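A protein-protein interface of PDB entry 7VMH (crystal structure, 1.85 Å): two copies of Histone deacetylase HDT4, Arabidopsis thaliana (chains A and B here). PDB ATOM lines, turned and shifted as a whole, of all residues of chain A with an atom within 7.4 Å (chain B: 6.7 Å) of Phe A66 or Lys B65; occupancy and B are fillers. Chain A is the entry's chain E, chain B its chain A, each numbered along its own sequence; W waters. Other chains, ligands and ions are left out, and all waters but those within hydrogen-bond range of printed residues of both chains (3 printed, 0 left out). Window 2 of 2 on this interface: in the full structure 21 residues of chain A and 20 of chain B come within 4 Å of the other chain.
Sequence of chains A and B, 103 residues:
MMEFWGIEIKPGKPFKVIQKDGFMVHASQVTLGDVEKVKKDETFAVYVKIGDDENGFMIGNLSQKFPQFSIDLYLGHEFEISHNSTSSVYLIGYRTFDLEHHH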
ATOM      1  N   VAL A  30      15.299 -11.117  -6.265  1.00  0.00           N
ATOM      2  CA  VAL A  30      15.545 -11.430  -7.666  1.00  0.00           C
ATOM      3  C   VAL A  30      14.952 -12.817  -7.902  1.00  0.00           C
ATOM      4  O   VAL A  30      15.346 -13.787  -7.249  1.00  0.00           O
ATOM      5  CB  VAL A  30      17.052 -11.484  -7.944  1.00  0.00           C
ATOM      6  CG1 VAL A  30      17.316 -11.812  -9.424  1.00  0.00           C
ATOM      7  CG2 VAL A  30      17.712 -10.174  -7.529  1.00  0.00           C
ATOM      8  N   LEU A  32      13.349 -15.792 -10.837  1.00  0.00           N
ATOM      9  CA  LEU A  32      13.109 -16.343 -12.159  1.00  0.00           C
ATOM     10  C   LEU A  32      11.617 -16.463 -12.459  1.00  0.00           C
ATOM     11  O   LEU A  32      10.869 -17.055 -11.712  1.00  0.00           O
ATOM     12  CB  LEU A  32      13.711 -17.722 -12.281  1.00  0.00           C
ATOM     13  CG  LEU A  32      14.899 -18.040 -13.147  1.00  0.00           C
ATOM     14  CD1 LEU A  32      15.003 -19.566 -13.224  1.00  0.00           C
ATOM     15  CD2 LEU A  32      14.924 -17.370 -14.486  1.00  0.00           C
ATOM     16  N   VAL A  35      10.070 -20.851 -14.084  1.00  0.00           N
ATOM     17  CA  VAL A  35      11.044 -21.884 -13.836  1.00  0.00           C
ATOM     18  C   VAL A  35      10.907 -23.006 -14.860  1.00  0.00           C
ATOM     19  O   VAL A  35      11.905 -23.562 -15.266  1.00  0.00           O
ATOM     20  CB  VAL A  35      10.983 -22.399 -12.392  1.00  0.00           C
ATOM     21  CG1 VAL A  35      11.223 -21.243 -11.433  1.00  0.00           C
ATOM     22  CG2 VAL A  35       9.655 -23.084 -12.089  1.00  0.00           C
ATOM     23  N   THR A  43      22.849 -22.467 -15.479  1.00  0.00           N
ATOM     24  CA  THR A  43      22.877 -21.349 -14.556  1.00  0.00           C
ATOM     25  C   THR A  43      23.006 -20.044 -15.291  1.00  0.00           C
ATOM     26  O   THR A  43      23.825 -19.936 -16.195  1.00  0.00           O
ATOM     27  CB  THR A  43      24.023 -21.511 -13.549  1.00  0.00           C
ATOM     28  OG1 THR A  43      23.758 -22.684 -12.800  1.00  0.00           O
ATOM     29  CG2 THR A  43      24.087 -20.335 -12.579  1.00  0.00           C
ATOM     30  N   ASN A  61      23.221 -15.459  -9.385  1.00  0.00           N
ATOM     31  CA  ASN A  61      22.876 -16.434 -10.391  1.00  0.00           C
ATOM     32  C   ASN A  61      21.540 -16.969 -10.114  1.00  0.00           C
ATOM     33  O   ASN A  61      21.099 -16.934  -8.963  1.00  0.00           O
ATOM     34  CB  ASN A  61      23.888 -17.628 -10.364  1.00  0.00           C
ATOM     35  CG  ASN A  61      25.268 -17.190 -10.737  1.00  0.00           C
ATOM     36  OD1 ASN A  61      25.568 -17.090 -11.922  1.00  0.00           O
ATOM     37  ND2 ASN A  61      26.113 -17.029  -9.773  1.00  0.00           N
ATOM     38  N   LEU A  62      20.884 -17.496 -11.168  1.00  0.00           N
ATOM     39  CA  LEU A  62      19.591 -18.132 -11.098  1.00  0.00           C
ATOM     40  C   LEU A  62      19.619 -19.421 -11.901  1.00  0.00           C
ATOM     41  O   LEU A  62      20.398 -19.552 -12.871  1.00  0.00           O
ATOM     42  CB  LEU A  62      18.528 -17.240 -11.714  1.00  0.00           C
ATOM     43  CG  LEU A  62      18.244 -15.915 -11.012  1.00  0.00           C
ATOM     44  CD1 LEU A  62      17.330 -15.096 -11.867  1.00  0.00           C
ATOM     45  CD2 LEU A  62      17.615 -16.147  -9.649  1.00  0.00           C
ATOM     46  N   SER A  63      18.741 -20.354 -11.516  1.00  0.00           N
ATOM     47  CA  SER A  63      18.558 -21.625 -12.248  1.00  0.00           C
ATOM     48  C   SER A  63      17.239 -22.222 -11.788  1.00  0.00           C
ATOM     49  O   SER A  63      16.652 -21.801 -10.781  1.00  0.00           O
ATOM     50  CB  SER A  63      19.676 -22.607 -11.922  1.00  0.00           C
ATOM     51  OG  SER A  63      19.709 -22.927 -10.554  1.00  0.00           O
ATOM     52  N   GLN A  64      16.777 -23.238 -12.509  1.00  0.00           N
ATOM     53  CA  GLN A  64      15.535 -23.944 -12.150  1.00  0.00           C
ATOM     54  C   GLN A  64      15.657 -24.452 -10.714  1.00  0.00           C
ATOM     55  O   GLN A  64      14.722 -24.365  -9.933  1.00  0.00           O
ATOM     56  CB  GLN A  64      15.313 -25.149 -13.104  1.00  0.00           C
ATOM     57  CG  GLN A  64      13.854 -25.374 -13.503  1.00  0.00           C
ATOM     58  CD  GLN A  64      13.722 -26.404 -14.609  1.00  0.00           C
ATOM     59  OE1 GLN A  64      14.276 -27.455 -14.462  1.00  0.00           O
ATOM     60  NE2 GLN A  64      12.980 -26.110 -15.711  1.00  0.00           N
ATOM     61  N   LYS A  65      16.844 -24.984 -10.372  1.00  0.00           N
ATOM     62  CA  LYS A  65      17.069 -25.543  -9.059  1.00  0.00           C
ATOM     63  C   LYS A  65      17.209 -24.520  -7.934  1.00  0.00           C
ATOM     64  O   LYS A  65      16.918 -24.872  -6.807  1.00  0.00           O
ATOM     65  CB  LYS A  65      18.277 -26.478  -9.106  1.00  0.00           C
ATOM     66  CG  LYS A  65      17.906 -27.804  -9.804  1.00  0.00           C
ATOM     67  CD  LYS A  65      19.140 -28.582 -10.193  1.00  0.00           C
ATOM     68  CE  LYS A  65      18.799 -29.601 -11.262  1.00  0.00           C
ATOM     69  NZ  LYS A  65      18.435 -28.957 -12.571  1.00  0.00           N
ATOM     70  N   PHE A  66      17.690 -23.301  -8.247  1.00  0.00           N
ATOM     71  CA  PHE A  66      17.838 -22.221  -7.282  1.00  0.00           C
ATOM     72  C   PHE A  66      17.257 -20.966  -7.957  1.00  0.00           C
ATOM     73  O   PHE A  66      17.982 -20.143  -8.518  1.00  0.00           O
ATOM     74  CB  PHE A  66      19.345 -22.074  -6.941  1.00  0.00           C
ATOM     75  CG  PHE A  66      19.654 -21.477  -5.589  1.00  0.00           C
ATOM     76  CD1 PHE A  66      19.000 -20.346  -5.097  1.00  0.00           C
ATOM     77  CD2 PHE A  66      20.736 -21.996  -4.844  1.00  0.00           C
ATOM     78  CE1 PHE A  66      19.379 -19.761  -3.911  1.00  0.00           C
ATOM     79  CE2 PHE A  66      21.108 -21.421  -3.635  1.00  0.00           C
ATOM     80  CZ  PHE A  66      20.415 -20.300  -3.170  1.00  0.00           C
ATOM     81  N   PRO A  67      15.920 -20.826  -8.011  1.00  0.00           N
ATOM     82  CA  PRO A  67      15.270 -19.847  -8.888  1.00  0.00           C
ATOM     83  C   PRO A  67      14.993 -18.455  -8.307  1.00  0.00           C
ATOM     84  O   PRO A  67      14.287 -17.684  -8.964  1.00  0.00           O
ATOM     85  CB  PRO A  67      13.941 -20.555  -9.189  1.00  0.00           C
ATOM     86  CG  PRO A  67      13.605 -21.257  -7.862  1.00  0.00           C
ATOM     87  CD  PRO A  67      14.957 -21.727  -7.358  1.00  0.00           C
ATOM     88  N   GLN A  68      15.520 -18.162  -7.113  1.00  0.00           N
ATOM     89  CA  GLN A  68      15.414 -16.821  -6.564  1.00  0.00           C
ATOM     90  C   GLN A  68      16.401 -16.638  -5.437  1.00  0.00           C
ATOM     91  O   GLN A  68      16.916 -17.604  -4.894  1.00  0.00           O
ATOM     92  CB  GLN A  68      13.996 -16.509  -6.059  1.00  0.00           C
ATOM     93  CG  GLN A  68      13.593 -17.290  -4.825  1.00  0.00           C
ATOM     94  CD  GLN A  68      12.142 -17.668  -4.817  1.00  0.00           C
ATOM     95  OE1 GLN A  68      11.402 -17.674  -5.828  1.00  0.00           O
ATOM     96  NE2 GLN A  68      11.711 -17.988  -3.635  1.00  0.00           N
ATOM     97  N   PHE A  69      16.725 -15.379  -5.134  1.00  0.00           N
ATOM     98  CA  PHE A  69      17.507 -15.061  -3.955  1.00  0.00           C
ATOM     99  C   PHE A  69      17.131 -13.672  -3.490  1.00  0.00           C
ATOM    100  O   PHE A  69      16.729 -12.822  -4.273  1.00  0.00           O
ATOM    101  CB  PHE A  69      19.012 -15.167  -4.226  1.00  0.00           C
ATOM    102  CG  PHE A  69      19.487 -14.314  -5.359  1.00  0.00           C
ATOM    103  CD1 PHE A  69      19.834 -12.997  -5.166  1.00  0.00           C
ATOM    104  CD2 PHE A  69      19.568 -14.858  -6.659  1.00  0.00           C
ATOM    105  CE1 PHE A  69      20.297 -12.237  -6.235  1.00  0.00           C
ATOM    106  CE2 PHE A  69      20.004 -14.090  -7.716  1.00  0.00           C
ATOM    107  CZ  PHE A  69      20.336 -12.782  -7.511  1.00  0.00           C
ATOM    108  N   SER A  70      17.271 -13.452  -2.180  1.00  0.00           N
ATOM    109  CA  SER A  70      17.092 -12.174  -1.544  1.00  0.00           C
ATOM    110  C   SER A  70      18.422 -11.424  -1.559  1.00  0.00           C
ATOM    111  O   SER A  70      19.498 -12.021  -1.607  1.00  0.00           O
ATOM    112  CB  SER A  70      16.564 -12.326  -0.098  1.00  0.00           C
ATOM    113  OG  SER A  70      17.500 -12.957   0.703  1.00  0.00           O
ATOM    114  N   LEU B  32      29.451 -16.124  -7.405  1.00  0.00           N
ATOM    115  CA  LEU B  32      30.397 -16.861  -8.218  1.00  0.00           C
ATOM    116  C   LEU B  32      30.221 -16.510  -9.685  1.00  0.00           C
ATOM    117  O   LEU B  32      29.107 -16.626 -10.212  1.00  0.00           O
ATOM    118  CB  LEU B  32      30.159 -18.355  -8.027  1.00  0.00           C
ATOM    119  CG  LEU B  32      31.187 -19.301  -8.677  1.00  0.00           C
ATOM    120  CD1 LEU B  32      32.612 -19.106  -8.224  1.00  0.00           C
ATOM    121  CD2 LEU B  32      30.719 -20.715  -8.380  1.00  0.00           C
ATOM    122  N   VAL B  35      29.631 -19.547 -13.720  1.00  0.00           N
ATOM    123  CA  VAL B  35      29.214 -20.768 -13.079  1.00  0.00           C
ATOM    124  C   VAL B  35      29.300 -21.967 -14.009  1.00  0.00           C
ATOM    125  O   VAL B  35      29.677 -23.051 -13.572  1.00  0.00           O
ATOM    126  CB  VAL B  35      27.813 -20.654 -12.439  1.00  0.00           C
ATOM    127  CG1 VAL B  35      27.332 -22.005 -11.917  1.00  0.00           C
ATOM    128  CG2 VAL B  35      27.869 -19.705 -11.253  1.00  0.00           C
ATOM    129  N   LYS B  39      34.348 -26.296 -12.207  1.00  0.00           N
ATOM    130  CA  LYS B  39      34.122 -27.723 -12.073  1.00  0.00           C
ATOM    131  C   LYS B  39      32.882 -27.923 -11.212  1.00  0.00           C
ATOM    132  O   LYS B  39      32.735 -27.309 -10.161  1.00  0.00           O
ATOM    133  CB  LYS B  39      35.374 -28.422 -11.497  1.00  0.00           C
ATOM    134  CG  LYS B  39      36.683 -27.919 -12.112  1.00  0.00           C
ATOM    135  CD  LYS B  39      37.666 -29.014 -12.453  1.00  0.00           C
ATOM    136  CE  LYS B  39      38.650 -28.504 -13.498  1.00  0.00           C
ATOM    137  NZ  LYS B  39      39.691 -29.510 -13.813  1.00  0.00           N
ATOM    138  N   LYS B  40      32.016 -28.839 -11.639  1.00  0.00           N
ATOM    139  CA  LYS B  40      30.695 -29.031 -11.051  1.00  0.00           C
ATOM    140  C   LYS B  40      30.675 -29.474  -9.577  1.00  0.00           C
ATOM    141  O   LYS B  40      29.714 -29.215  -8.886  1.00  0.00           O
ATOM    142  CB  LYS B  40      29.920 -30.061 -11.893  1.00  0.00           C
ATOM    143  CG  LYS B  40      29.581 -29.619 -13.305  1.00  0.00           C
ATOM    144  CD  LYS B  40      28.232 -28.940 -13.342  1.00  0.00           C
ATOM    145  CE  LYS B  40      27.875 -28.533 -14.754  1.00  0.00           C
ATOM    146  NZ  LYS B  40      28.777 -27.455 -15.254  1.00  0.00           N
ATOM    147  N   ASP B  41      31.747 -30.125  -9.113  1.00  0.00           N
ATOM    148  CA  ASP B  41      31.862 -30.721  -7.825  1.00  0.00           C
ATOM    149  C   ASP B  41      32.849 -30.030  -6.864  1.00  0.00           C
ATOM    150  O   ASP B  41      33.199 -30.597  -5.855  1.00  0.00           O
ATOM    151  CB  ASP B  41      32.405 -32.142  -8.076  1.00  0.00           C
ATOM    152  CG  ASP B  41      33.765 -32.121  -8.822  1.00  0.00           C
ATOM    153  OD1 ASP B  41      33.839 -31.432  -9.841  1.00  0.00           O
ATOM    154  OD2 ASP B  41      34.749 -32.724  -8.395  1.00  0.00           O
ATOM    155  N   GLU B  42      33.293 -28.815  -7.197  1.00  0.00           N
ATOM    156  CA  GLU B  42      34.179 -28.052  -6.343  1.00  0.00           C
ATOM    157  C   GLU B  42      33.372 -27.148  -5.398  1.00  0.00           C
ATOM    158  O   GLU B  42      32.335 -26.649  -5.783  1.00  0.00           O
ATOM    159  CB  GLU B  42      35.106 -27.169  -7.190  1.00  0.00           C
ATOM    160  CG  GLU B  42      36.108 -27.910  -8.075  1.00  0.00           C
ATOM    161  CD  GLU B  42      37.097 -28.768  -7.302  1.00  0.00           C
ATOM    162  OE1 GLU B  42      37.411 -28.400  -6.133  1.00  0.00           O
ATOM    163  OE2 GLU B  42      37.541 -29.819  -7.867  1.00  0.00           O
ATOM    164  N   THR B  43      33.887 -26.919  -4.189  1.00  0.00           N
ATOM    165  CA  THR B  43      33.462 -25.801  -3.355  1.00  0.00           C
ATOM    166  C   THR B  43      34.627 -24.852  -3.223  1.00  0.00           C
ATOM    167  O   THR B  43      35.768 -25.279  -2.967  1.00  0.00           O
ATOM    168  CB  THR B  43      33.013 -26.256  -1.968  1.00  0.00           C
ATOM    169  OG1 THR B  43      31.874 -27.099  -2.143  1.00  0.00           O
ATOM    170  CG2 THR B  43      32.590 -25.092  -1.097  1.00  0.00           C
ATOM    171  N   LEU B  62      31.250 -20.992  -2.033  1.00  0.00           N
ATOM    172  CA  LEU B  62      30.555 -20.906  -3.308  1.00  0.00           C
ATOM    173  C   LEU B  62      30.736 -22.196  -4.069  1.00  0.00           C
ATOM    174  O   LEU B  62      31.786 -22.819  -4.016  1.00  0.00           O
ATOM    175  CB  LEU B  62      31.155 -19.775  -4.162  1.00  0.00           C
ATOM    176  CG  LEU B  62      30.969 -18.362  -3.638  1.00  0.00           C
ATOM    177  CD1 LEU B  62      31.853 -17.377  -4.371  1.00  0.00           C
ATOM    178  CD2 LEU B  62      29.504 -17.997  -3.748  1.00  0.00           C
ATOM    179  N   SER B  63      29.713 -22.566  -4.835  1.00  0.00           N
ATOM    180  CA  SER B  63      29.789 -23.749  -5.714  1.00  0.00           C
ATOM    181  C   SER B  63      28.742 -23.572  -6.786  1.00  0.00           C
ATOM    182  O   SER B  63      27.868 -22.709  -6.701  1.00  0.00           O
ATOM    183  CB  SER B  63      29.508 -25.014  -4.931  1.00  0.00           C
ATOM    184  OG  SER B  63      28.199 -24.953  -4.333  1.00  0.00           O
ATOM    185  N   GLN B  64      28.812 -24.435  -7.801  1.00  0.00           N
ATOM    186  CA  GLN B  64      27.824 -24.380  -8.876  1.00  0.00           C
ATOM    187  C   GLN B  64      26.415 -24.572  -8.296  1.00  0.00           C
ATOM    188  O   GLN B  64      25.492 -23.927  -8.704  1.00  0.00           O
ATOM    189  CB  GLN B  64      28.154 -25.397  -9.937  1.00  0.00           C
ATOM    190  CG  GLN B  64      27.122 -25.428 -11.046  1.00  0.00           C
ATOM    191  CD  GLN B  64      26.155 -26.564 -10.879  1.00  0.00           C
ATOM    192  OE1 GLN B  64      26.388 -27.508 -10.122  1.00  0.00           O
ATOM    193  NE2 GLN B  64      25.074 -26.505 -11.630  1.00  0.00           N
ATOM    194  N   LYS B  65      26.295 -25.428  -7.298  1.00  0.00           N
ATOM    195  CA  LYS B  65      25.009 -25.696  -6.655  1.00  0.00           C
ATOM    196  C   LYS B  65      24.509 -24.603  -5.730  1.00  0.00           C
ATOM    197  O   LYS B  65      23.304 -24.467  -5.587  1.00  0.00           O
ATOM    198  CB  LYS B  65      25.037 -27.041  -5.895  1.00  0.00           C
ATOM    199  CG  LYS B  65      26.246 -27.365  -4.991  1.00  0.00           C
ATOM    200  CD  LYS B  65      26.908 -28.712  -5.371  1.00  0.00           C
ATOM    201  CE  LYS B  65      27.455 -28.656  -6.809  1.00  0.00           C
ATOM    202  NZ  LYS B  65      28.590 -27.712  -6.955  1.00  0.00           N
ATOM    203  N   PHE B  66      25.426 -23.842  -5.103  1.00  0.00           N
ATOM    204  CA  PHE B  66      25.078 -22.730  -4.196  1.00  0.00           C
ATOM    205  C   PHE B  66      25.970 -21.557  -4.639  1.00  0.00           C
ATOM    206  O   PHE B  66      27.005 -21.309  -4.048  1.00  0.00           O
ATOM    207  CB  PHE B  66      25.316 -23.168  -2.747  1.00  0.00           C
ATOM    208  CG  PHE B  66      24.506 -22.433  -1.682  1.00  0.00           C
ATOM    209  CD1 PHE B  66      24.371 -21.048  -1.667  1.00  0.00           C
ATOM    210  CD2 PHE B  66      23.975 -23.155  -0.606  1.00  0.00           C
ATOM    211  CE1 PHE B  66      23.740 -20.400  -0.618  1.00  0.00           C
ATOM    212  CE2 PHE B  66      23.296 -22.538   0.422  1.00  0.00           C
ATOM    213  CZ  PHE B  66      23.184 -21.134   0.432  1.00  0.00           C
ATOM    214  N   PRO B  67      25.644 -20.884  -5.761  1.00  0.00           N
ATOM    215  CA  PRO B  67      26.572 -19.971  -6.430  1.00  0.00           C
ATOM    216  C   PRO B  67      26.529 -18.499  -6.034  1.00  0.00           C
ATOM    217  O   PRO B  67      27.148 -17.664  -6.716  1.00  0.00           O
ATOM    218  CB  PRO B  67      26.122 -20.114  -7.904  1.00  0.00           C
ATOM    219  CG  PRO B  67      24.627 -20.284  -7.806  1.00  0.00           C
ATOM    220  CD  PRO B  67      24.419 -21.106  -6.554  1.00  0.00           C
ATOM    221  N   GLN B  68      25.819 -18.189  -4.949  1.00  0.00           N
ATOM    222  CA  GLN B  68      25.901 -16.868  -4.340  1.00  0.00           C
ATOM    223  C   GLN B  68      25.346 -16.974  -2.918  1.00  0.00           C
ATOM    224  O   GLN B  68      24.602 -17.891  -2.610  1.00  0.00           O
ATOM    225  CB  GLN B  68      25.120 -15.816  -5.165  1.00  0.00           C
ATOM    226  CG  GLN B  68      23.597 -15.985  -5.082  1.00  0.00           C
ATOM    227  CD  GLN B  68      23.052 -17.034  -5.998  1.00  0.00           C
ATOM    228  OE1 GLN B  68      23.448 -17.099  -7.186  1.00  0.00           O
ATOM    229  NE2 GLN B  68      22.166 -17.876  -5.475  1.00  0.00           N
HETATM  230  O   HOH W   1      23.637 -22.884 -10.179  1.00  0.00           O
HETATM  231  O   HOH W   2      27.862 -17.249 -13.551  1.00  0.00           O
HETATM  232  O   HOH W   3      20.912 -19.349  -7.724  1.00  0.00           O
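Hydrophobic or aromatic side chains of chain A within 4 Å of the printed part of chain B: Phe A66. Printed residues of chain B that touch a printed residue of chain A: Leu B32, Val B35, Lys B65, Phe B66, Pro B67 and Gln B68. Hydrophobic or aromatic side chains of chain B within 4 Å of the printed part of chain A: Val B35, Phe B66 and Pro B67. Among the printed residues, 8 pairs touch across the chains. Among the printed residues, no Asp or Glu carboxylate lies within 4 Å of a Lys or Arg side-chain nitrogen of the other chain.
ND2 of Asn A61 is in hydrogen-bond range of O of Pro B67 (3.3 Å). O of Leu B32 lies within hydrogen-bond range of ND2 of Asn A61. The side-chain amide oxygen of Gln B68 is in hydrogen-bond range of the backbone NH of Asn A61.
The side-chain hydroxyl (OG) of Ser B63 sits at hydrogen-bond distance from the backbone NH (N) of Phe B66 (3.1 Å). O of Lys B40 lies within hydrogen-bond range of NZ of Lys B65 (2.7 Å). N of Leu B32 sits at hydrogen-bond distance from O of Pro B67 (2.9 Å). The backbone NH (N) of Phe A66 lies within hydrogen-bond range of the side-chain hydroxyl (OG) of Ser A63.
Thr A43 touches Val B35, but with the chains exchanged Val A35 does not touch Thr B43 (23.4 Å). Phe A66 touches Lys B65, but with the chains exchanged Lys A65 does not touch Phe B66 (8.6 Å). Phe A66 touches its own counterpart, Phe B66. Phe A66 touches Gln B68, but with the chains exchanged Gln A68 does not touch Phe B66 (8.5 Å). Of the 8 pairs that touch across the chains among the printed residues, 1 has its exchanged pair printed and touching as well.
Water W1 lies within hydrogen-bond range of the backbone carbonyl oxygen (O) of Gln B64 (2.6 Å) and the side-chain hydroxyl (OG1) of Thr A43 (2.6 Å). Water W3 lies within hydrogen-bond range of the backbone carbonyl oxygen (O) of Asn A61 (2.7 Å), the side-chain amide nitrogen (NE2) of Gln B68 (3.0 Å) and the backbone carbonyl oxygen (O) of Phe A66 (3.1 Å). Water W2 lies within hydrogen-bond range of OD1 of Asn A61 (2.8 Å) and N of Val B35 (2.9 Å).
Of chain B, only Lys B65 (3.6 Å), Phe B66 (3.8 Å) and Gln B68 (3.7 Å) come within 4 Å of Phe A66. Lys B65 touches just one residue of chain A: Phe A66. Printed residues of chain A within 4 Å of Val B35: Thr A43 (3.7 Å) and Asn A61 (3.5 Å). Of the printed residues of chain A, Gln B68 touches Asn A61 and Phe A66. Of the printed residues of chain A, Leu B32 touches Asn A61 (3.1 Å). Printed residues of chain B within 4 Å of Thr A43: Val B35 (3.7 Å). Phe A69 touches none of the printed residues of chain B. Gln A68 touches none of the printed residues of chain B. The nearest residue of chain A that does not touch Lys B65 is Ser A63 (6.3 Å).
Among the printed residues, merely in contact across the chains: Thr A43 with Val B35, Asn A61 with Val B35, Phe A66 with Lys B65, Phe A66 with Phe B66 and Phe A66 with Gln B68.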
